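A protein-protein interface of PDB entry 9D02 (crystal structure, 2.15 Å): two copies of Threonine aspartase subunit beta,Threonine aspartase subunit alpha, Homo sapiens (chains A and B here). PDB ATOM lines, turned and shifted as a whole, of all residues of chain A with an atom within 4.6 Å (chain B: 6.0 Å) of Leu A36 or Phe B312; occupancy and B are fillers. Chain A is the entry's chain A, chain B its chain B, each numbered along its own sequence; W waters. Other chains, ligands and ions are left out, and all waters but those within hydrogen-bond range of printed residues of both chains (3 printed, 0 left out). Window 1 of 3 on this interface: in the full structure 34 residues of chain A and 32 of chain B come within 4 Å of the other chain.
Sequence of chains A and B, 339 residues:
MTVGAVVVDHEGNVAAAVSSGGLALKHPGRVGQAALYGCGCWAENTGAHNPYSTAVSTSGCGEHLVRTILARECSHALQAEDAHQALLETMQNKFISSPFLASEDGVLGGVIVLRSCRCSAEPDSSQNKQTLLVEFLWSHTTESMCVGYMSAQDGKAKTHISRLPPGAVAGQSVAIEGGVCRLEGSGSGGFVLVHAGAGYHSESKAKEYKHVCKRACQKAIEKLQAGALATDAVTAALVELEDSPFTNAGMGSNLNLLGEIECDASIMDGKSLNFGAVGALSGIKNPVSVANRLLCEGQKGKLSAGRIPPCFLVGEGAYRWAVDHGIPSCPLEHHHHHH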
ATOM      1  N   GLY A  29      33.618   4.304 -22.441  1.00  0.00           N
ATOM      2  CA  GLY A  29      32.230   4.186 -22.029  1.00  0.00           C
ATOM      3  C   GLY A  29      31.380   3.254 -22.873  1.00  0.00           C
ATOM      4  O   GLY A  29      30.184   3.096 -22.580  1.00  0.00           O
ATOM      5  N   ARG A  30      31.939   2.628 -23.908  1.00  0.00           N
ATOM      6  CA  ARG A  30      31.159   1.661 -24.677  1.00  0.00           C
ATOM      7  C   ARG A  30      30.952   0.389 -23.869  1.00  0.00           C
ATOM      8  O   ARG A  30      31.914  -0.223 -23.402  1.00  0.00           O
ATOM      9  CB  ARG A  30      31.842   1.330 -26.002  1.00  0.00           C
ATOM     10  CG  ARG A  30      31.059   0.262 -26.841  1.00  0.00           C
ATOM     11  CD  ARG A  30      31.737  -0.009 -28.210  1.00  0.00           C
ATOM     12  NE  ARG A  30      30.936  -0.913 -29.039  1.00  0.00           N
ATOM     13  CZ  ARG A  30      30.934  -0.917 -30.368  1.00  0.00           C
ATOM     14  NH1 ARG A  30      31.688  -0.059 -31.043  1.00  0.00           N
ATOM     15  NH2 ARG A  30      30.151  -1.762 -31.028  1.00  0.00           N
ATOM     16  N   VAL A  31      29.698  -0.024 -23.728  1.00  0.00           N
ATOM     17  CA  VAL A  31      29.331  -1.237 -23.002  1.00  0.00           C
ATOM     18  C   VAL A  31      28.768  -2.248 -24.002  1.00  0.00           C
ATOM     19  O   VAL A  31      27.961  -1.880 -24.861  1.00  0.00           O
ATOM     20  CB  VAL A  31      28.308  -0.922 -21.898  1.00  0.00           C
ATOM     21  CG1 VAL A  31      27.815  -2.194 -21.244  1.00  0.00           C
ATOM     22  CG2 VAL A  31      28.932   0.005 -20.849  1.00  0.00           C
ATOM     23  N   GLY A  32      29.207  -3.507 -23.904  1.00  0.00           N
ATOM     24  CA  GLY A  32      28.756  -4.579 -24.797  1.00  0.00           C
ATOM     25  C   GLY A  32      28.011  -5.671 -24.060  1.00  0.00           C
ATOM     26  O   GLY A  32      27.586  -5.461 -22.911  1.00  0.00           O
ATOM     27  N   GLN A  33      27.921  -6.866 -24.656  1.00  0.00           N
ATOM     28  CA  GLN A  33      26.936  -7.855 -24.214  1.00  0.00           C
ATOM     29  C   GLN A  33      27.236  -8.429 -22.834  1.00  0.00           C
ATOM     30  O   GLN A  33      26.310  -8.858 -22.140  1.00  0.00           O
ATOM     31  CB  GLN A  33      26.829  -9.006 -25.216  1.00  0.00           C
ATOM     32  CG  GLN A  33      27.488 -10.296 -24.770  1.00  0.00           C
ATOM     33  CD  GLN A  33      28.907 -10.343 -25.214  1.00  0.00           C
ATOM     34  OE1 GLN A  33      29.389  -9.388 -25.806  1.00  0.00           O
ATOM     35  NE2 GLN A  33      29.592 -11.457 -24.958  1.00  0.00           N
ATOM     36  N   ALA A  34      28.504  -8.471 -22.431  1.00  0.00           N
ATOM     37  CA  ALA A  34      28.877  -9.102 -21.164  1.00  0.00           C
ATOM     38  C   ALA A  34      28.276  -8.391 -19.951  1.00  0.00           C
ATOM     39  O   ALA A  34      28.294  -8.943 -18.842  1.00  0.00           O
ATOM     40  CB  ALA A  34      30.405  -9.120 -21.024  1.00  0.00           C
ATOM     41  N   ALA A  35      27.799  -7.164 -20.118  1.00  0.00           N
ATOM     42  CA  ALA A  35      27.163  -6.438 -19.024  1.00  0.00           C
ATOM     43  C   ALA A  35      25.639  -6.448 -19.102  1.00  0.00           C
ATOM     44  O   ALA A  35      24.989  -5.975 -18.167  1.00  0.00           O
ATOM     45  CB  ALA A  35      27.637  -4.983 -19.013  1.00  0.00           C
ATOM     46  N   LEU A  36      25.052  -6.932 -20.190  1.00  0.00           N
ATOM     47  CA  LEU A  36      23.660  -6.612 -20.481  1.00  0.00           C
ATOM     48  C   LEU A  36      22.756  -7.784 -20.141  1.00  0.00           C
ATOM     49  O   LEU A  36      22.998  -8.918 -20.585  1.00  0.00           O
ATOM     50  CB  LEU A  36      23.488  -6.194 -21.939  1.00  0.00           C
ATOM     51  CG  LEU A  36      24.285  -4.939 -22.277  1.00  0.00           C
ATOM     52  CD1 LEU A  36      24.055  -4.556 -23.729  1.00  0.00           C
ATOM     53  CD2 LEU A  36      23.857  -3.829 -21.373  1.00  0.00           C
ATOM     54  N   TYR A  37      21.737  -7.500 -19.329  1.00  0.00           N
ATOM     55  CA  TYR A  37      20.749  -8.497 -18.935  1.00  0.00           C
ATOM     56  C   TYR A  37      20.151  -9.219 -20.136  1.00  0.00           C
ATOM     57  O   TYR A  37      19.705  -8.589 -21.098  1.00  0.00           O
ATOM     58  CB  TYR A  37      19.652  -7.791 -18.147  1.00  0.00           C
ATOM     59  CG  TYR A  37      18.644  -8.703 -17.517  1.00  0.00           C
ATOM     60  CD1 TYR A  37      18.994  -9.547 -16.464  1.00  0.00           C
ATOM     61  CD2 TYR A  37      17.325  -8.699 -17.949  1.00  0.00           C
ATOM     62  CE1 TYR A  37      18.044 -10.369 -15.864  1.00  0.00           C
ATOM     63  CE2 TYR A  37      16.377  -9.518 -17.356  1.00  0.00           C
ATOM     64  CZ  TYR A  37      16.738 -10.348 -16.323  1.00  0.00           C
ATOM     65  OH  TYR A  37      15.780 -11.149 -15.761  1.00  0.00           O
ATOM     66  N   GLY A  38      20.108 -10.549 -20.061  1.00  0.00           N
ATOM     67  CA  GLY A  38      19.603 -11.360 -21.144  1.00  0.00           C
ATOM     68  C   GLY A  38      20.589 -11.644 -22.260  1.00  0.00           C
ATOM     69  O   GLY A  38      20.402 -12.622 -22.999  1.00  0.00           O
ATOM     70  N   CYS A  39      21.631 -10.832 -22.422  1.00  0.00           N
ATOM     71  CA  CYS A  39      22.493 -10.932 -23.595  1.00  0.00           C
ATOM     72  C   CYS A  39      23.751 -11.743 -23.316  1.00  0.00           C
ATOM     73  O   CYS A  39      24.026 -12.734 -24.005  1.00  0.00           O
ATOM     74  CB  CYS A  39      22.866  -9.520 -24.077  1.00  0.00           C
ATOM     75  SG  CYS A  39      21.379  -8.491 -24.454  1.00  0.00           S
ATOM     76  N   GLY A  40      24.486 -11.376 -22.271  1.00  0.00           N
ATOM     77  CA  GLY A  40      25.762 -11.996 -21.992  1.00  0.00           C
ATOM     78  C   GLY A  40      25.646 -13.348 -21.325  1.00  0.00           C
ATOM     79  O   GLY A  40      26.429 -14.250 -21.639  1.00  0.00           O
ATOM     80  N   VAL A  66      24.238  -8.708 -28.434  1.00  0.00           N
ATOM     81  CA  VAL A  66      23.236  -7.829 -27.839  1.00  0.00           C
ATOM     82  C   VAL A  66      21.947  -7.845 -28.657  1.00  0.00           C
ATOM     83  O   VAL A  66      20.867  -8.118 -28.124  1.00  0.00           O
ATOM     84  CB  VAL A  66      23.796  -6.405 -27.691  1.00  0.00           C
ATOM     85  CG1 VAL A  66      22.737  -5.435 -27.075  1.00  0.00           C
ATOM     86  CG2 VAL A  66      25.076  -6.434 -26.856  1.00  0.00           C
ATOM     87  N   PHE A 275      20.479 -11.061 -10.469  1.00  0.00           N
ATOM     88  CA  PHE A 275      21.437 -10.712 -11.507  1.00  0.00           C
ATOM     89  C   PHE A 275      22.305  -9.575 -10.982  1.00  0.00           C
ATOM     90  O   PHE A 275      21.799  -8.692 -10.284  1.00  0.00           O
ATOM     91  CB  PHE A 275      20.660 -10.280 -12.765  1.00  0.00           C
ATOM     92  CG  PHE A 275      21.503  -9.706 -13.887  1.00  0.00           C
ATOM     93  CD1 PHE A 275      22.124 -10.541 -14.823  1.00  0.00           C
ATOM     94  CD2 PHE A 275      21.613  -8.321 -14.048  1.00  0.00           C
ATOM     95  CE1 PHE A 275      22.871 -10.006 -15.882  1.00  0.00           C
ATOM     96  CE2 PHE A 275      22.342  -7.777 -15.093  1.00  0.00           C
ATOM     97  CZ  PHE A 275      22.979  -8.630 -16.024  1.00  0.00           C
ATOM     98  N   PHE A 312      23.022  -3.188 -11.613  1.00  0.00           N
ATOM     99  CA  PHE A 312      23.865  -2.834 -12.754  1.00  0.00           C
ATOM    100  C   PHE A 312      24.521  -1.490 -12.468  1.00  0.00           C
ATOM    101  O   PHE A 312      23.838  -0.462 -12.435  1.00  0.00           O
ATOM    102  CB  PHE A 312      23.022  -2.770 -14.041  1.00  0.00           C
ATOM    103  CG  PHE A 312      23.815  -2.465 -15.291  1.00  0.00           C
ATOM    104  CD1 PHE A 312      25.160  -2.772 -15.372  1.00  0.00           C
ATOM    105  CD2 PHE A 312      23.202  -1.871 -16.391  1.00  0.00           C
ATOM    106  CE1 PHE A 312      25.884  -2.492 -16.549  1.00  0.00           C
ATOM    107  CE2 PHE A 312      23.911  -1.588 -17.554  1.00  0.00           C
ATOM    108  CZ  PHE A 312      25.257  -1.901 -17.632  1.00  0.00           C
ATOM    109  N   VAL B  31      22.384   2.082 -13.393  1.00  0.00           N
ATOM    110  CA  VAL B  31      21.673   2.164 -14.659  1.00  0.00           C
ATOM    111  C   VAL B  31      20.442   1.272 -14.579  1.00  0.00           C
ATOM    112  O   VAL B  31      20.540   0.118 -14.150  1.00  0.00           O
ATOM    113  CB  VAL B  31      22.592   1.752 -15.817  1.00  0.00           C
ATOM    114  CG1 VAL B  31      21.806   1.703 -17.131  1.00  0.00           C
ATOM    115  CG2 VAL B  31      23.782   2.695 -15.884  1.00  0.00           C
ATOM    116  N   ALA B  35      17.893   2.505 -20.242  1.00  0.00           N
ATOM    117  CA  ALA B  35      19.076   2.391 -21.090  1.00  0.00           C
ATOM    118  C   ALA B  35      19.258   1.010 -21.696  1.00  0.00           C
ATOM    119  O   ALA B  35      20.176   0.837 -22.495  1.00  0.00           O
ATOM    120  CB  ALA B  35      20.369   2.732 -20.313  1.00  0.00           C
ATOM    121  N   LEU B  36      18.460   0.020 -21.307  1.00  0.00           N
ATOM    122  CA  LEU B  36      18.805  -1.370 -21.570  1.00  0.00           C
ATOM    123  C   LEU B  36      18.005  -1.898 -22.756  1.00  0.00           C
ATOM    124  O   LEU B  36      16.770  -1.825 -22.765  1.00  0.00           O
ATOM    125  CB  LEU B  36      18.547  -2.231 -20.340  1.00  0.00           C
ATOM    126  CG  LEU B  36      19.324  -1.806 -19.092  1.00  0.00           C
ATOM    127  CD1 LEU B  36      19.006  -2.776 -17.958  1.00  0.00           C
ATOM    128  CD2 LEU B  36      20.807  -1.788 -19.415  1.00  0.00           C
ATOM    129  N   TYR B  37      18.724  -2.417 -23.742  1.00  0.00           N
ATOM    130  CA  TYR B  37      18.136  -3.045 -24.920  1.00  0.00           C
ATOM    131  C   TYR B  37      17.078  -4.065 -24.515  1.00  0.00           C
ATOM    132  O   TYR B  37      17.287  -4.856 -23.593  1.00  0.00           O
ATOM    133  CB  TYR B  37      19.254  -3.722 -25.716  1.00  0.00           C
ATOM    134  CG  TYR B  37      18.813  -4.277 -27.061  1.00  0.00           C
ATOM    135  CD1 TYR B  37      18.408  -3.418 -28.081  1.00  0.00           C
ATOM    136  CD2 TYR B  37      18.827  -5.649 -27.315  1.00  0.00           C
ATOM    137  CE1 TYR B  37      18.020  -3.900 -29.317  1.00  0.00           C
ATOM    138  CE2 TYR B  37      18.434  -6.151 -28.565  1.00  0.00           C
ATOM    139  CZ  TYR B  37      18.044  -5.266 -29.557  1.00  0.00           C
ATOM    140  OH  TYR B  37      17.677  -5.734 -30.794  1.00  0.00           O
ATOM    141  N   PHE B 275      19.539   0.695 -32.822  1.00  0.00           N
ATOM    142  CA  PHE B 275      19.294   1.055 -31.436  1.00  0.00           C
ATOM    143  C   PHE B 275      20.412   1.986 -30.971  1.00  0.00           C
ATOM    144  O   PHE B 275      21.560   1.844 -31.404  1.00  0.00           O
ATOM    145  CB  PHE B 275      19.237  -0.229 -30.603  1.00  0.00           C
ATOM    146  CG  PHE B 275      19.118  -0.015 -29.123  1.00  0.00           C
ATOM    147  CD1 PHE B 275      17.880   0.226 -28.551  1.00  0.00           C
ATOM    148  CD2 PHE B 275      20.231  -0.134 -28.296  1.00  0.00           C
ATOM    149  CE1 PHE B 275      17.753   0.390 -27.182  1.00  0.00           C
ATOM    150  CE2 PHE B 275      20.117   0.025 -26.923  1.00  0.00           C
ATOM    151  CZ  PHE B 275      18.883   0.291 -26.368  1.00  0.00           C
ATOM    152  N   GLY B 276      20.068   2.958 -30.138  1.00  0.00           N
ATOM    153  CA  GLY B 276      21.069   3.788 -29.481  1.00  0.00           C
ATOM    154  C   GLY B 276      20.694   3.981 -28.028  1.00  0.00           C
ATOM    155  O   GLY B 276      19.515   3.995 -27.677  1.00  0.00           O
ATOM    156  N   ALA B 277      21.705   4.133 -27.171  1.00  0.00           N
ATOM    157  CA  ALA B 277      21.377   4.216 -25.753  1.00  0.00           C
ATOM    158  C   ALA B 277      22.497   4.900 -24.969  1.00  0.00           C
ATOM    159  O   ALA B 277      23.676   4.802 -25.326  1.00  0.00           O
ATOM    160  CB  ALA B 277      21.083   2.822 -25.189  1.00  0.00           C
ATOM    161  N   VAL B 278      22.106   5.631 -23.917  1.00  0.00           N
ATOM    162  CA  VAL B 278      23.055   6.171 -22.951  1.00  0.00           C
ATOM    163  C   VAL B 278      22.628   5.788 -21.542  1.00  0.00           C
ATOM    164  O   VAL B 278      21.435   5.706 -21.233  1.00  0.00           O
ATOM    165  CB  VAL B 278      23.207   7.709 -23.084  1.00  0.00           C
ATOM    166  CG1 VAL B 278      23.847   8.048 -24.424  1.00  0.00           C
ATOM    167  CG2 VAL B 278      21.839   8.416 -22.939  1.00  0.00           C
ATOM    168  N   GLY B 279      23.619   5.597 -20.674  1.00  0.00           N
ATOM    169  CA  GLY B 279      23.360   5.308 -19.275  1.00  0.00           C
ATOM    170  C   GLY B 279      24.265   6.143 -18.387  1.00  0.00           C
ATOM    171  O   GLY B 279      25.397   6.472 -18.750  1.00  0.00           O
ATOM    172  N   LEU B 294      23.636   8.410 -31.561  1.00  0.00           N
ATOM    173  CA  LEU B 294      24.281   7.100 -31.659  1.00  0.00           C
ATOM    174  C   LEU B 294      23.587   6.225 -32.699  1.00  0.00           C
ATOM    175  O   LEU B 294      24.251   5.554 -33.503  1.00  0.00           O
ATOM    176  CB  LEU B 294      24.267   6.408 -30.290  1.00  0.00           C
ATOM    177  CG  LEU B 294      25.297   6.919 -29.272  1.00  0.00           C
ATOM    178  CD1 LEU B 294      24.913   6.495 -27.848  1.00  0.00           C
ATOM    179  CD2 LEU B 294      26.707   6.431 -29.614  1.00  0.00           C
ATOM    180  N   PRO B 310      29.384   2.120 -32.061  1.00  0.00           N
ATOM    181  CA  PRO B 310      28.792   1.905 -30.737  1.00  0.00           C
ATOM    182  C   PRO B 310      27.311   2.237 -30.724  1.00  0.00           C
ATOM    183  O   PRO B 310      26.859   3.178 -31.377  1.00  0.00           O
ATOM    184  CB  PRO B 310      29.563   2.882 -29.847  1.00  0.00           C
ATOM    185  CG  PRO B 310      29.884   4.015 -30.796  1.00  0.00           C
ATOM    186  CD  PRO B 310      30.245   3.317 -32.081  1.00  0.00           C
ATOM    187  N   CYS B 311      26.554   1.455 -29.959  1.00  0.00           N
ATOM    188  CA  CYS B 311      25.157   1.749 -29.744  1.00  0.00           C
ATOM    189  C   CYS B 311      24.822   2.088 -28.295  1.00  0.00           C
ATOM    190  O   CYS B 311      23.770   2.676 -28.055  1.00  0.00           O
ATOM    191  CB  CYS B 311      24.295   0.566 -30.207  1.00  0.00           C
ATOM    192  SG  CYS B 311      24.372  -0.850 -29.131  1.00  0.00           S
ATOM    193  N   PHE B 312      25.682   1.743 -27.335  1.00  0.00           N
ATOM    194  CA  PHE B 312      25.415   1.954 -25.911  1.00  0.00           C
ATOM    195  C   PHE B 312      26.656   2.548 -25.246  1.00  0.00           C
ATOM    196  O   PHE B 312      27.675   1.859 -25.115  1.00  0.00           O
ATOM    197  CB  PHE B 312      25.021   0.623 -25.249  1.00  0.00           C
ATOM    198  CG  PHE B 312      24.663   0.740 -23.769  1.00  0.00           C
ATOM    199  CD1 PHE B 312      24.178   1.926 -23.241  1.00  0.00           C
ATOM    200  CD2 PHE B 312      24.813  -0.351 -22.923  1.00  0.00           C
ATOM    201  CE1 PHE B 312      23.832   2.030 -21.882  1.00  0.00           C
ATOM    202  CE2 PHE B 312      24.472  -0.269 -21.575  1.00  0.00           C
ATOM    203  CZ  PHE B 312      23.990   0.922 -21.043  1.00  0.00           C
ATOM    204  N   LEU B 313      26.582   3.827 -24.821  1.00  0.00           N
ATOM    205  CA  LEU B 313      27.669   4.505 -24.110  1.00  0.00           C
ATOM    206  C   LEU B 313      27.207   4.960 -22.729  1.00  0.00           C
ATOM    207  O   LEU B 313      26.044   5.331 -22.543  1.00  0.00           O
ATOM    208  CB  LEU B 313      28.194   5.735 -24.884  1.00  0.00           C
ATOM    209  CG  LEU B 313      28.768   5.535 -26.288  1.00  0.00           C
ATOM    210  CD1 LEU B 313      29.148   6.871 -26.899  1.00  0.00           C
ATOM    211  CD2 LEU B 313      29.978   4.594 -26.234  1.00  0.00           C
ATOM    212  N   VAL B 314      28.130   4.955 -21.758  1.00  0.00           N
ATOM    213  CA  VAL B 314      27.800   5.349 -20.393  1.00  0.00           C
ATOM    214  C   VAL B 314      28.807   6.356 -19.848  1.00  0.00           C
ATOM    215  O   VAL B 314      29.947   6.456 -20.315  1.00  0.00           O
ATOM    216  CB  VAL B 314      27.709   4.141 -19.438  1.00  0.00           C
ATOM    217  CG1 VAL B 314      26.654   3.152 -19.921  1.00  0.00           C
ATOM    218  CG2 VAL B 314      29.090   3.466 -19.274  1.00  0.00           C
HETATM  219  O   HOH W   1      19.333  -5.682 -21.709  1.00  0.00           O
HETATM  220  O   HOH W   2      20.428  -1.256 -11.546  1.00  0.00           O
HETATM  221  O   HOH W   3      27.751  -0.356 -27.661  1.00  0.00           O
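Hydrophobic or aromatic side chains of chain B that line the printed part of chain A: Val B31, Leu B36, Tyr B37, Pro B310, Phe B312, Leu B313 and Val B314. Of the 15 printed residues of chain A, 6 touch a printed residue of chain B. Printed residues of chain A that touch a printed residue of chain B: Gly A29, Arg A30, Val A31, Leu A36, Val A66 and Phe A312. Hydrophobic or aromatic side chains of chain A within 4 Å of the printed part of chain B: Val A31, Leu A36, Val A66 and Phe A312. Among the printed residues, 12 pairs touch across the chains. Among the printed residues, no Asp or Glu carboxylate lies within 4 Å of a Lys or Arg side-chain nitrogen of the other chain.
Val A31 touches Phe B312, and with the chains exchanged Phe A312 touches Val B31. Leu A36 touches Phe B312, and with the chains exchanged Phe A312 touches Leu B36.
The backbone NH (N) of Val B314 sits at hydrogen-bond distance from the backbone carbonyl oxygen (O) of Gly A29 (2.9 Å). The backbone carbonyl oxygen (O) of Phe B312 lies within hydrogen-bond range of the backbone NH (N) of Val A31 (3.1 Å). O of Phe A312 lies within hydrogen-bond range of N of Val B31 (3.1 Å). N of Pro B310 sits close to NH1 of Arg A30 (3.3 Å).
The side-chain sulfur of Cys A39 is in hydrogen-bond range of the backbone carbonyl oxygen of Val A66, at 3.7 Å. O of Ala B277 lies within hydrogen-bond range of N of Leu B313 (3.1 Å). O of Leu B313 is in hydrogen-bond range of N of Gly B279, at 3.1 Å.
Among the printed residues, pairs that only touch across the chains: Val A66 with Tyr B37 (3.2 Å), Gly A29 with Leu B313 (3.3 Å), Arg A30 with Phe B312 (3.5 Å), Arg A30 with Leu B313 (3.5 Å), Leu A36 with Phe B312 (3.6 Å), Phe A312 with Leu B36 (3.6 Å), Gly A29 with Phe B312 (3.8 Å) and Val A31 with Val B314 (3.8 Å).
Water W1 lies within hydrogen-bond range of O of Tyr B37 (2.9 Å) and O of Tyr A37 (3.0 Å). Water W2 lies within hydrogen-bond range of O of Val B31 and N of Phe A312. Water W3 lies within hydrogen-bond range of the backbone NH of Phe B312 (3.0 Å), the backbone NH of Cys B311 (3.2 Å) and the backbone carbonyl oxygen of Val A31 (3.2 Å).
Of chain B, only Phe B312 (3.6 Å) comes within 4 Å of Leu A36. Printed residues of chain A within 4 Å of Phe B312: Gly A29 (3.8 Å), Arg A30 (3.5 Å), Val A31 (3.1 Å) and Leu A36 (3.6 Å). Printed residues of chain A within 4 Å of Val B31: Phe A312 (3.1 Å). Printed residues of chain B within 4 Å of Val A66: Tyr B37. Printed residues of chain A within 4 Å of Tyr B37: Val A66 (3.2 Å). Phe B275 touches none of the printed residues of chain A. Gln A33 touches none of the printed residues of chain B. The nearest residue of chain A that does not touch Phe B312 is Phe A312 (4.3 Å). The nearest printed residue of chain B that does not touch Arg A30 is Cys B311 (4.9 Å).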
